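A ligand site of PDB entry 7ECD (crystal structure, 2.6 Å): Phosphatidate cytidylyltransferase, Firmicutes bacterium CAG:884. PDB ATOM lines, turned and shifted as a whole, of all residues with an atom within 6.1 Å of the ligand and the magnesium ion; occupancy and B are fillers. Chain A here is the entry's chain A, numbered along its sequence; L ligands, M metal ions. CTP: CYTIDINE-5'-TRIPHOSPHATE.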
ATOM      1  N   TYR A  28       4.484  10.743  20.176  1.00  0.00           N
ATOM      2  CA  TYR A  28       5.630  10.411  19.331  1.00  0.00           C
ATOM      3  C   TYR A  28       6.357   9.219  19.937  1.00  0.00           C
ATOM      4  O   TYR A  28       6.020   8.731  21.012  1.00  0.00           O
ATOM      5  CB  TYR A  28       6.572  11.616  19.182  1.00  0.00           C
ATOM      6  CG  TYR A  28       7.318  11.945  20.448  1.00  0.00           C
ATOM      7  CD1 TYR A  28       8.706  11.958  20.470  1.00  0.00           C
ATOM      8  CD2 TYR A  28       6.633  12.220  21.629  1.00  0.00           C
ATOM      9  CE1 TYR A  28       9.393  12.260  21.633  1.00  0.00           C
ATOM     10  CE2 TYR A  28       7.307  12.524  22.792  1.00  0.00           C
ATOM     11  CZ  TYR A  28       8.679  12.537  22.798  1.00  0.00           C
ATOM     12  OH  TYR A  28       9.337  12.827  23.970  1.00  0.00           O
ATOM     13  N   GLY A  29       7.355   8.727  19.221  1.00  0.00           N
ATOM     14  CA  GLY A  29       8.146   7.631  19.735  1.00  0.00           C
ATOM     15  C   GLY A  29       7.548   6.243  19.550  1.00  0.00           C
ATOM     16  O   GLY A  29       6.521   6.027  18.902  1.00  0.00           O
ATOM     17  N   SER A  30       8.231   5.266  20.174  1.00  0.00           N
ATOM     18  CA  SER A  30       7.963   3.853  19.939  1.00  0.00           C
ATOM     19  C   SER A  30       6.668   3.368  20.579  1.00  0.00           C
ATOM     20  O   SER A  30       6.242   2.254  20.301  1.00  0.00           O
ATOM     21  CB  SER A  30       9.115   3.008  20.479  1.00  0.00           C
ATOM     22  OG  SER A  30       9.026   2.920  21.889  1.00  0.00           O
ATOM     23  N   GLY A  31       6.072   4.148  21.454  1.00  0.00           N
ATOM     24  CA  GLY A  31       4.804   3.745  22.018  1.00  0.00           C
ATOM     25  C   GLY A  31       3.608   4.191  21.209  1.00  0.00           C
ATOM     26  O   GLY A  31       2.479   3.894  21.599  1.00  0.00           O
ATOM     27  N   GLN A  35       8.064   0.368  15.726  1.00  0.00           N
ATOM     28  CA  GLN A  35       9.477   0.338  15.396  1.00  0.00           C
ATOM     29  C   GLN A  35       9.876  -1.102  15.170  1.00  0.00           C
ATOM     30  O   GLN A  35       9.404  -2.000  15.872  1.00  0.00           O
ATOM     31  CB  GLN A  35      10.281   0.958  16.529  1.00  0.00           C
ATOM     32  CG  GLN A  35      10.879   2.314  16.281  1.00  0.00           C
ATOM     33  CD  GLN A  35      11.650   2.804  17.497  1.00  0.00           C
ATOM     34  OE1 GLN A  35      12.624   2.175  17.941  1.00  0.00           O
ATOM     35  NE2 GLN A  35      11.185   3.914  18.059  1.00  0.00           N
ATOM     36  N   TYR A  38      11.986  -4.383  18.124  1.00  0.00           N
ATOM     37  CA  TYR A  38      11.523  -4.685  19.465  1.00  0.00           C
ATOM     38  C   TYR A  38      11.085  -6.128  19.443  1.00  0.00           C
ATOM     39  O   TYR A  38      10.393  -6.565  18.514  1.00  0.00           O
ATOM     40  CB  TYR A  38      10.347  -3.785  19.899  1.00  0.00           C
ATOM     41  CG  TYR A  38      10.744  -2.386  20.313  1.00  0.00           C
ATOM     42  CD1 TYR A  38      11.006  -1.409  19.354  1.00  0.00           C
ATOM     43  CD2 TYR A  38      10.863  -2.035  21.656  1.00  0.00           C
ATOM     44  CE1 TYR A  38      11.373  -0.120  19.725  1.00  0.00           C
ATOM     45  CE2 TYR A  38      11.229  -0.760  22.035  1.00  0.00           C
ATOM     46  CZ  TYR A  38      11.480   0.203  21.060  1.00  0.00           C
ATOM     47  OH  TYR A  38      11.853   1.486  21.420  1.00  0.00           O
ATOM     48  N   PRO A  44       6.625  -0.650  25.641  1.00  0.00           N
ATOM     49  CA  PRO A  44       7.339   0.618  25.740  1.00  0.00           C
ATOM     50  C   PRO A  44       6.420   1.739  26.199  1.00  0.00           C
ATOM     51  O   PRO A  44       5.199   1.641  26.158  1.00  0.00           O
ATOM     52  CB  PRO A  44       7.853   0.857  24.310  1.00  0.00           C
ATOM     53  CG  PRO A  44       6.972   0.066  23.454  1.00  0.00           C
ATOM     54  CD  PRO A  44       6.491  -1.112  24.255  1.00  0.00           C
ATOM     55  N   GLN A  45       7.052   2.813  26.683  1.00  0.00           N
ATOM     56  CA  GLN A  45       6.315   3.942  27.204  1.00  0.00           C
ATOM     57  C   GLN A  45       5.661   4.741  26.092  1.00  0.00           C
ATOM     58  O   GLN A  45       6.190   4.844  24.976  1.00  0.00           O
ATOM     59  CB  GLN A  45       7.231   4.858  28.008  1.00  0.00           C
ATOM     60  CG  GLN A  45       7.222   4.538  29.464  1.00  0.00           C
ATOM     61  CD  GLN A  45       8.198   5.372  30.256  1.00  0.00           C
ATOM     62  OE1 GLN A  45       7.816   6.071  31.177  1.00  0.00           O
ATOM     63  NE2 GLN A  45       9.473   5.280  29.908  1.00  0.00           N
ATOM     64  N   ILE A  46       4.500   5.310  26.391  1.00  0.00           N
ATOM     65  CA  ILE A  46       3.817   6.239  25.493  1.00  0.00           C
ATOM     66  C   ILE A  46       4.403   7.626  25.726  1.00  0.00           C
ATOM     67  O   ILE A  46       4.234   8.200  26.799  1.00  0.00           O
ATOM     68  CB  ILE A  46       2.301   6.231  25.712  1.00  0.00           C
ATOM     69  CG1 ILE A  46       1.695   4.906  25.239  1.00  0.00           C
ATOM     70  CG2 ILE A  46       1.668   7.381  24.964  1.00  0.00           C
ATOM     71  CD1 ILE A  46       0.288   4.676  25.734  1.00  0.00           C
ATOM     72  N   ASP A  47       5.113   8.152  24.732  1.00  0.00           N
ATOM     73  CA  ASP A  47       5.826   9.412  24.843  1.00  0.00           C
ATOM     74  C   ASP A  47       4.951  10.539  24.296  1.00  0.00           C
ATOM     75  O   ASP A  47       4.464  10.450  23.169  1.00  0.00           O
ATOM     76  CB  ASP A  47       7.152   9.411  24.056  1.00  0.00           C
ATOM     77  CG  ASP A  47       8.085   8.255  24.427  1.00  0.00           C
ATOM     78  OD1 ASP A  47       8.367   7.417  23.559  1.00  0.00           O
ATOM     79  OD2 ASP A  47       8.547   8.188  25.575  1.00  0.00           O
ATOM     80  N   LYS A 106       4.959   8.864  29.478  1.00  0.00           N
ATOM     81  CA  LYS A 106       6.054   9.788  29.766  1.00  0.00           C
ATOM     82  C   LYS A 106       5.809  11.047  28.960  1.00  0.00           C
ATOM     83  O   LYS A 106       5.872  11.015  27.718  1.00  0.00           O
ATOM     84  CB  LYS A 106       7.407   9.175  29.430  1.00  0.00           C
ATOM     85  CG  LYS A 106       8.504  10.192  29.287  1.00  0.00           C
ATOM     86  CD  LYS A 106       9.734   9.643  28.631  1.00  0.00           C
ATOM     87  CE  LYS A 106      10.972  10.157  29.344  1.00  0.00           C
ATOM     88  NZ  LYS A 106      12.173  10.273  28.481  1.00  0.00           N
ATOM     89  N   TYR A 126      16.854  20.081  20.796  1.00  0.00           N
ATOM     90  CA  TYR A 126      16.332  18.877  21.423  1.00  0.00           C
ATOM     91  C   TYR A 126      14.901  18.597  20.969  1.00  0.00           C
ATOM     92  O   TYR A 126      14.602  17.522  20.433  1.00  0.00           O
ATOM     93  CB  TYR A 126      16.406  19.031  22.932  1.00  0.00           C
ATOM     94  CG  TYR A 126      16.143  17.746  23.655  1.00  0.00           C
ATOM     95  CD1 TYR A 126      14.843  17.368  23.968  1.00  0.00           C
ATOM     96  CD2 TYR A 126      17.196  16.921  24.036  1.00  0.00           C
ATOM     97  CE1 TYR A 126      14.599  16.196  24.646  1.00  0.00           C
ATOM     98  CE2 TYR A 126      16.974  15.759  24.712  1.00  0.00           C
ATOM     99  CZ  TYR A 126      15.667  15.385  25.019  1.00  0.00           C
ATOM    100  OH  TYR A 126      15.441  14.196  25.681  1.00  0.00           O
ATOM    101  N   GLY A 129      14.276  18.450  16.973  1.00  0.00           N
ATOM    102  CA  GLY A 129      14.745  17.223  16.372  1.00  0.00           C
ATOM    103  C   GLY A 129      13.737  16.112  16.514  1.00  0.00           C
ATOM    104  O   GLY A 129      13.596  15.268  15.630  1.00  0.00           O
ATOM    105  N   ARG A 130      13.012  16.094  17.635  1.00  0.00           N
ATOM    106  CA  ARG A 130      11.990  15.084  17.830  1.00  0.00           C
ATOM    107  C   ARG A 130      10.814  15.293  16.879  1.00  0.00           C
ATOM    108  O   ARG A 130      10.137  14.333  16.495  1.00  0.00           O
ATOM    109  CB  ARG A 130      11.527  15.078  19.280  1.00  0.00           C
ATOM    110  CG  ARG A 130      12.330  14.143  20.153  1.00  0.00           C
ATOM    111  CD  ARG A 130      13.104  14.892  21.226  1.00  0.00           C
ATOM    112  NE  ARG A 130      13.875  13.954  22.049  1.00  0.00           N
ATOM    113  CZ  ARG A 130      15.194  13.961  22.147  1.00  0.00           C
ATOM    114  NH1 ARG A 130      15.895  14.891  21.489  1.00  0.00           N
ATOM    115  NH2 ARG A 130      15.810  13.068  22.911  1.00  0.00           N
ATOM    116  N   PHE A 131      10.584  16.541  16.475  1.00  0.00           N
ATOM    117  CA  PHE A 131       9.487  16.851  15.571  1.00  0.00           C
ATOM    118  C   PHE A 131       9.846  16.603  14.112  1.00  0.00           C
ATOM    119  O   PHE A 131       9.000  16.852  13.226  1.00  0.00           O
ATOM    120  CB  PHE A 131       9.054  18.301  15.810  1.00  0.00           C
ATOM    121  CG  PHE A 131       8.045  18.421  16.905  1.00  0.00           C
ATOM    122  CD1 PHE A 131       6.697  18.445  16.606  1.00  0.00           C
ATOM    123  CD2 PHE A 131       8.443  18.450  18.231  1.00  0.00           C
ATOM    124  CE1 PHE A 131       5.749  18.515  17.627  1.00  0.00           C
ATOM    125  CE2 PHE A 131       7.497  18.529  19.257  1.00  0.00           C
ATOM    126  CZ  PHE A 131       6.150  18.569  18.951  1.00  0.00           C
ATOM    127  N   LYS A 133      10.566  13.483  13.274  1.00  0.00           N
ATOM    128  CA  LYS A 133      10.129  12.113  13.116  1.00  0.00           C
ATOM    129  C   LYS A 133       8.600  12.108  13.096  1.00  0.00           C
ATOM    130  O   LYS A 133       7.992  13.173  13.249  1.00  0.00           O
ATOM    131  CB  LYS A 133      10.684  11.250  14.248  1.00  0.00           C
ATOM    132  CG  LYS A 133      12.148  10.883  14.061  1.00  0.00           C
ATOM    133  CD  LYS A 133      12.995  11.963  14.686  1.00  0.00           C
ATOM    134  CE  LYS A 133      14.470  11.792  14.387  1.00  0.00           C
ATOM    135  NZ  LYS A 133      15.146  13.148  14.372  1.00  0.00           N
ATOM    136  N   PRO A 134       7.947  10.972  12.884  1.00  0.00           N
ATOM    137  CA  PRO A 134       6.483  10.960  12.901  1.00  0.00           C
ATOM    138  C   PRO A 134       5.928  11.608  14.162  1.00  0.00           C
ATOM    139  O   PRO A 134       6.457  11.419  15.261  1.00  0.00           O
ATOM    140  CB  PRO A 134       6.130   9.474  12.850  1.00  0.00           C
ATOM    141  CG  PRO A 134       7.256   8.872  12.109  1.00  0.00           C
ATOM    142  CD  PRO A 134       8.480   9.644  12.494  1.00  0.00           C
ATOM    143  N   CYS A 176      16.594  11.676   9.837  1.00  0.00           N
ATOM    144  CA  CYS A 176      16.171  11.106  11.091  1.00  0.00           C
ATOM    145  C   CYS A 176      17.335  11.017  12.074  1.00  0.00           C
ATOM    146  O   CYS A 176      17.129  10.829  13.278  1.00  0.00           O
ATOM    147  CB  CYS A 176      15.542   9.748  10.793  1.00  0.00           C
ATOM    148  SG  CYS A 176      15.262   8.746  12.234  1.00  0.00           S
ATOM    149  N   SER A 179      19.202  14.570  15.079  1.00  0.00           N
ATOM    150  CA  SER A 179      19.101  14.719  16.520  1.00  0.00           C
ATOM    151  C   SER A 179      19.673  13.529  17.294  1.00  0.00           C
ATOM    152  O   SER A 179      19.628  13.529  18.527  1.00  0.00           O
ATOM    153  CB  SER A 179      17.640  14.953  16.933  1.00  0.00           C
ATOM    154  OG  SER A 179      16.854  13.809  16.667  1.00  0.00           O
ATOM    155  N   TYR A 180      20.188  12.529  16.598  1.00  0.00           N
ATOM    156  CA  TYR A 180      20.829  11.379  17.234  1.00  0.00           C
ATOM    157  C   TYR A 180      22.351  11.463  17.216  1.00  0.00           C
ATOM    158  O   TYR A 180      23.003  10.823  18.052  1.00  0.00           O
ATOM    159  CB  TYR A 180      20.372  10.072  16.580  1.00  0.00           C
ATOM    160  CG  TYR A 180      19.119   9.485  17.183  1.00  0.00           C
ATOM    161  CD1 TYR A 180      17.894   9.569  16.525  1.00  0.00           C
ATOM    162  CD2 TYR A 180      19.146   8.867  18.416  1.00  0.00           C
ATOM    163  CE1 TYR A 180      16.732   9.049  17.084  1.00  0.00           C
ATOM    164  CE2 TYR A 180      17.996   8.321  18.978  1.00  0.00           C
ATOM    165  CZ  TYR A 180      16.801   8.425  18.315  1.00  0.00           C
ATOM    166  OH  TYR A 180      15.674   7.889  18.874  1.00  0.00           O
ATOM    167  N   ASP A 183      24.174  12.019  20.634  1.00  0.00           N
ATOM    168  CA  ASP A 183      23.306  11.763  21.770  1.00  0.00           C
ATOM    169  C   ASP A 183      24.035  10.878  22.764  1.00  0.00           C
ATOM    170  O   ASP A 183      24.568   9.823  22.400  1.00  0.00           O
ATOM    171  CB  ASP A 183      22.006  11.105  21.300  1.00  0.00           C
ATOM    172  CG  ASP A 183      21.048  10.757  22.442  1.00  0.00           C
ATOM    173  OD1 ASP A 183      21.494  10.353  23.539  1.00  0.00           O
ATOM    174  OD2 ASP A 183      19.819  10.835  22.246  1.00  0.00           O
ATOM    175  N   MET A 186      22.420   6.923  24.164  1.00  0.00           N
ATOM    176  CA  MET A 186      22.294   5.811  23.241  1.00  0.00           C
ATOM    177  C   MET A 186      23.618   5.077  23.160  1.00  0.00           C
ATOM    178  O   MET A 186      24.612   5.641  22.695  1.00  0.00           O
ATOM    179  CB  MET A 186      21.913   6.299  21.838  1.00  0.00           C
ATOM    180  CG  MET A 186      20.525   6.896  21.724  1.00  0.00           C
ATOM    181  SD  MET A 186      19.273   5.671  21.338  1.00  0.00           S
ATOM    182  CE  MET A 186      20.134   4.630  20.167  1.00  0.00           C
ATOM    183  N   LYS A 194      18.846   2.192  15.703  1.00  0.00           N
ATOM    184  CA  LYS A 194      17.646   2.916  16.108  1.00  0.00           C
ATOM    185  C   LYS A 194      17.084   3.727  14.948  1.00  0.00           C
ATOM    186  O   LYS A 194      15.877   3.675  14.666  1.00  0.00           O
ATOM    187  CB  LYS A 194      17.956   3.838  17.292  1.00  0.00           C
ATOM    188  CG  LYS A 194      16.730   4.426  17.937  1.00  0.00           C
ATOM    189  CD  LYS A 194      15.915   3.335  18.565  1.00  0.00           C
ATOM    190  CE  LYS A 194      14.872   3.875  19.506  1.00  0.00           C
ATOM    191  NZ  LYS A 194      14.148   2.728  20.104  1.00  0.00           N
ATOM    192  N   ILE A 198      13.507   3.100  12.875  1.00  0.00           N
ATOM    193  CA  ILE A 198      12.437   4.088  12.837  1.00  0.00           C
ATOM    194  C   ILE A 198      11.969   4.297  11.404  1.00  0.00           C
ATOM    195  O   ILE A 198      10.765   4.269  11.120  1.00  0.00           O
ATOM    196  CB  ILE A 198      12.907   5.407  13.465  1.00  0.00           C
ATOM    197  CG1 ILE A 198      12.874   5.315  14.995  1.00  0.00           C
ATOM    198  CG2 ILE A 198      12.068   6.567  12.952  1.00  0.00           C
ATOM    199  CD1 ILE A 198      13.608   6.482  15.681  1.00  0.00           C
ATOM    200  N   ASN A 257      23.391  18.215  20.491  1.00  0.00           N
ATOM    201  CA  ASN A 257      22.759  16.967  20.908  1.00  0.00           C
ATOM    202  C   ASN A 257      23.484  16.360  22.091  1.00  0.00           C
ATOM    203  O   ASN A 257      22.851  15.757  22.973  1.00  0.00           O
ATOM    204  CB  ASN A 257      22.723  15.995  19.741  1.00  0.00           C
ATOM    205  CG  ASN A 257      21.789  16.443  18.639  1.00  0.00           C
ATOM    206  OD1 ASN A 257      20.748  17.075  18.892  1.00  0.00           O
ATOM    207  ND2 ASN A 257      22.135  16.101  17.402  1.00  0.00           N
HETATM  208  N1  CTP L   1      14.293  11.212  19.309  1.00  0.00           N
HETATM  209  C2  CTP L   1      15.072  11.984  18.495  1.00  0.00           C
HETATM  210  N3  CTP L   1      16.367  12.298  18.861  1.00  0.00           N
HETATM  211  C4  CTP L   1      16.958  11.653  19.918  1.00  0.00           C
HETATM  212  C5  CTP L   1      16.229  10.740  20.657  1.00  0.00           C
HETATM  213  C6  CTP L   1      14.899  10.524  20.335  1.00  0.00           C
HETATM  214  O2  CTP L   1      14.601  12.396  17.435  1.00  0.00           O
HETATM  215  N4  CTP L   1      18.221  11.922  20.204  1.00  0.00           N
HETATM  216  C1' CTP L   1      12.934  10.939  18.843  1.00  0.00           C
HETATM  217  C2' CTP L   1      12.823   9.562  18.260  1.00  0.00           C
HETATM  218  O2' CTP L   1      11.997   9.670  17.163  1.00  0.00           O
HETATM  219  C3' CTP L   1      12.140   8.755  19.345  1.00  0.00           C
HETATM  220  C4' CTP L   1      11.539   9.743  20.306  1.00  0.00           C
HETATM  221  O4' CTP L   1      12.051  10.988  19.926  1.00  0.00           O
HETATM  222  O3' CTP L   1      11.149   7.904  18.848  1.00  0.00           O
HETATM  223  C5' CTP L   1      12.217   9.560  21.627  1.00  0.00           C
HETATM  224  O5' CTP L   1      11.533   8.690  22.445  1.00  0.00           O
HETATM  225  PA  CTP L   1      12.491   7.681  23.200  1.00  0.00           P
HETATM  226  O1A CTP L   1      11.639   7.070  24.267  1.00  0.00           O
HETATM  227  O2A CTP L   1      13.792   8.276  23.572  1.00  0.00           O
HETATM  228  O3A CTP L   1      12.882   6.621  22.094  1.00  0.00           O
HETATM  229  PB  CTP L   1      11.897   5.393  21.765  1.00  0.00           P
HETATM  230  O1B CTP L   1      10.483   5.531  22.344  1.00  0.00           O
HETATM  231  O2B CTP L   1      12.020   5.387  20.264  1.00  0.00           O
HETATM  232  O3B CTP L   1      12.618   4.132  22.415  1.00  0.00           O
HETATM  233  PG  CTP L   1      12.186   3.581  23.848  1.00  0.00           P
HETATM  234  O1G CTP L   1      11.329   4.556  24.606  1.00  0.00           O
HETATM  235  O2G CTP L   1      11.424   2.289  23.703  1.00  0.00           O
HETATM  236  O3G CTP L   1      13.477   3.316  24.570  1.00  0.00           O
HETATM  237 MG    MG M   1       9.897   6.277  24.498  1.00  0.00          MG
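The backbone NH of Ser 30 lies close to an oxygen (O1B) of the ligand (3.1 Å). The side-chain hydroxyl (OG) of Ser 30 lies within hydrogen-bond range of an oxygen (O2G) of the ligand. NZ of Lys 133 lies close to O2 of the ligand (3.2 Å). NE2 of Gln 35 is in hydrogen-bond range of O2B of the ligand, 2.8 Å away. The side-chain hydroxyl (OG) of Ser 179 sits at hydrogen-bond distance from a nitrogen (N3) of the ligand (2.7 Å). The side-chain amino group (NZ) of Lys 194 is in salt-bridge range of an oxygen (O2B) of the ligand (3.4 Å). O of Ser 179 sits at hydrogen-bond distance from N4 of the ligand, 2.7 Å away. The side-chain carboxylate of Asp 183 sits at hydrogen-bond distance from a nitrogen (N4) of the ligand (2.8 Å). OH of Tyr 38 is in hydrogen-bond range of O2G of the ligand (2.5 Å).
An oxygen (O1A) of the ligand is bound to the magnesium ion (1.9 Å). OD1 of Asp 47 is bound to the magnesium ion (2.1 Å). O1G of the ligand binds the magnesium ion, 2.2 Å away. An oxygen (O1B) of the ligand is bound to the magnesium ion, at 2.4 Å. OD2 of Asp 47 binds the magnesium ion, at 2.6 Å.
One residue has an atom within 4 Å of the magnesium ion: Asp 47. The nearest printed residue that does not touch the magnesium ion is Gln 45 (4.003 Å).
NZ of Lys 194 sits at hydrogen-bond distance from OH of Tyr 38, 2.9 Å away. OH of Tyr 38 sits at hydrogen-bond distance from OG of Ser 30 (3.2 Å). NH2 of Arg 130 sits at hydrogen-bond distance from OH of Tyr 126 (3.0 Å). The side-chain amino group of Lys 133 lies close to the backbone carbonyl oxygen of Cys 176, 3.2 Å away. The backbone carbonyl oxygen (O) of Asp 47 is in hydrogen-bond range of the backbone NH (N) of Tyr 28, 3.0 Å away. The backbone carbonyl oxygen of Gly 129 lies within hydrogen-bond range of the side-chain amino group of Lys 133 (2.9 Å). The side-chain amino group (NZ) of Lys 133 is in hydrogen-bond range of the side-chain hydroxyl (OG) of Ser 179 (2.9 Å). The side-chain amide oxygen of Gln 35 is in hydrogen-bond range of the side-chain amino group of Lys 194, 2.7 Å away.
Residues that only touch the ligand: Tyr 28, Gly 29, Pro 44, Gly 129, Arg 130, Tyr 180 and Ile 198. Hydrophobic or aromatic side chains within 4 Å of the ligand: Tyr 28, Tyr 38, Pro 44, Tyr 180 and Ile 198. Of the 25 residues printed, 15 come within 4 Å of the ligand. The nearest printed residue that does not touch the ligand is Gly 31 (4.7 Å).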
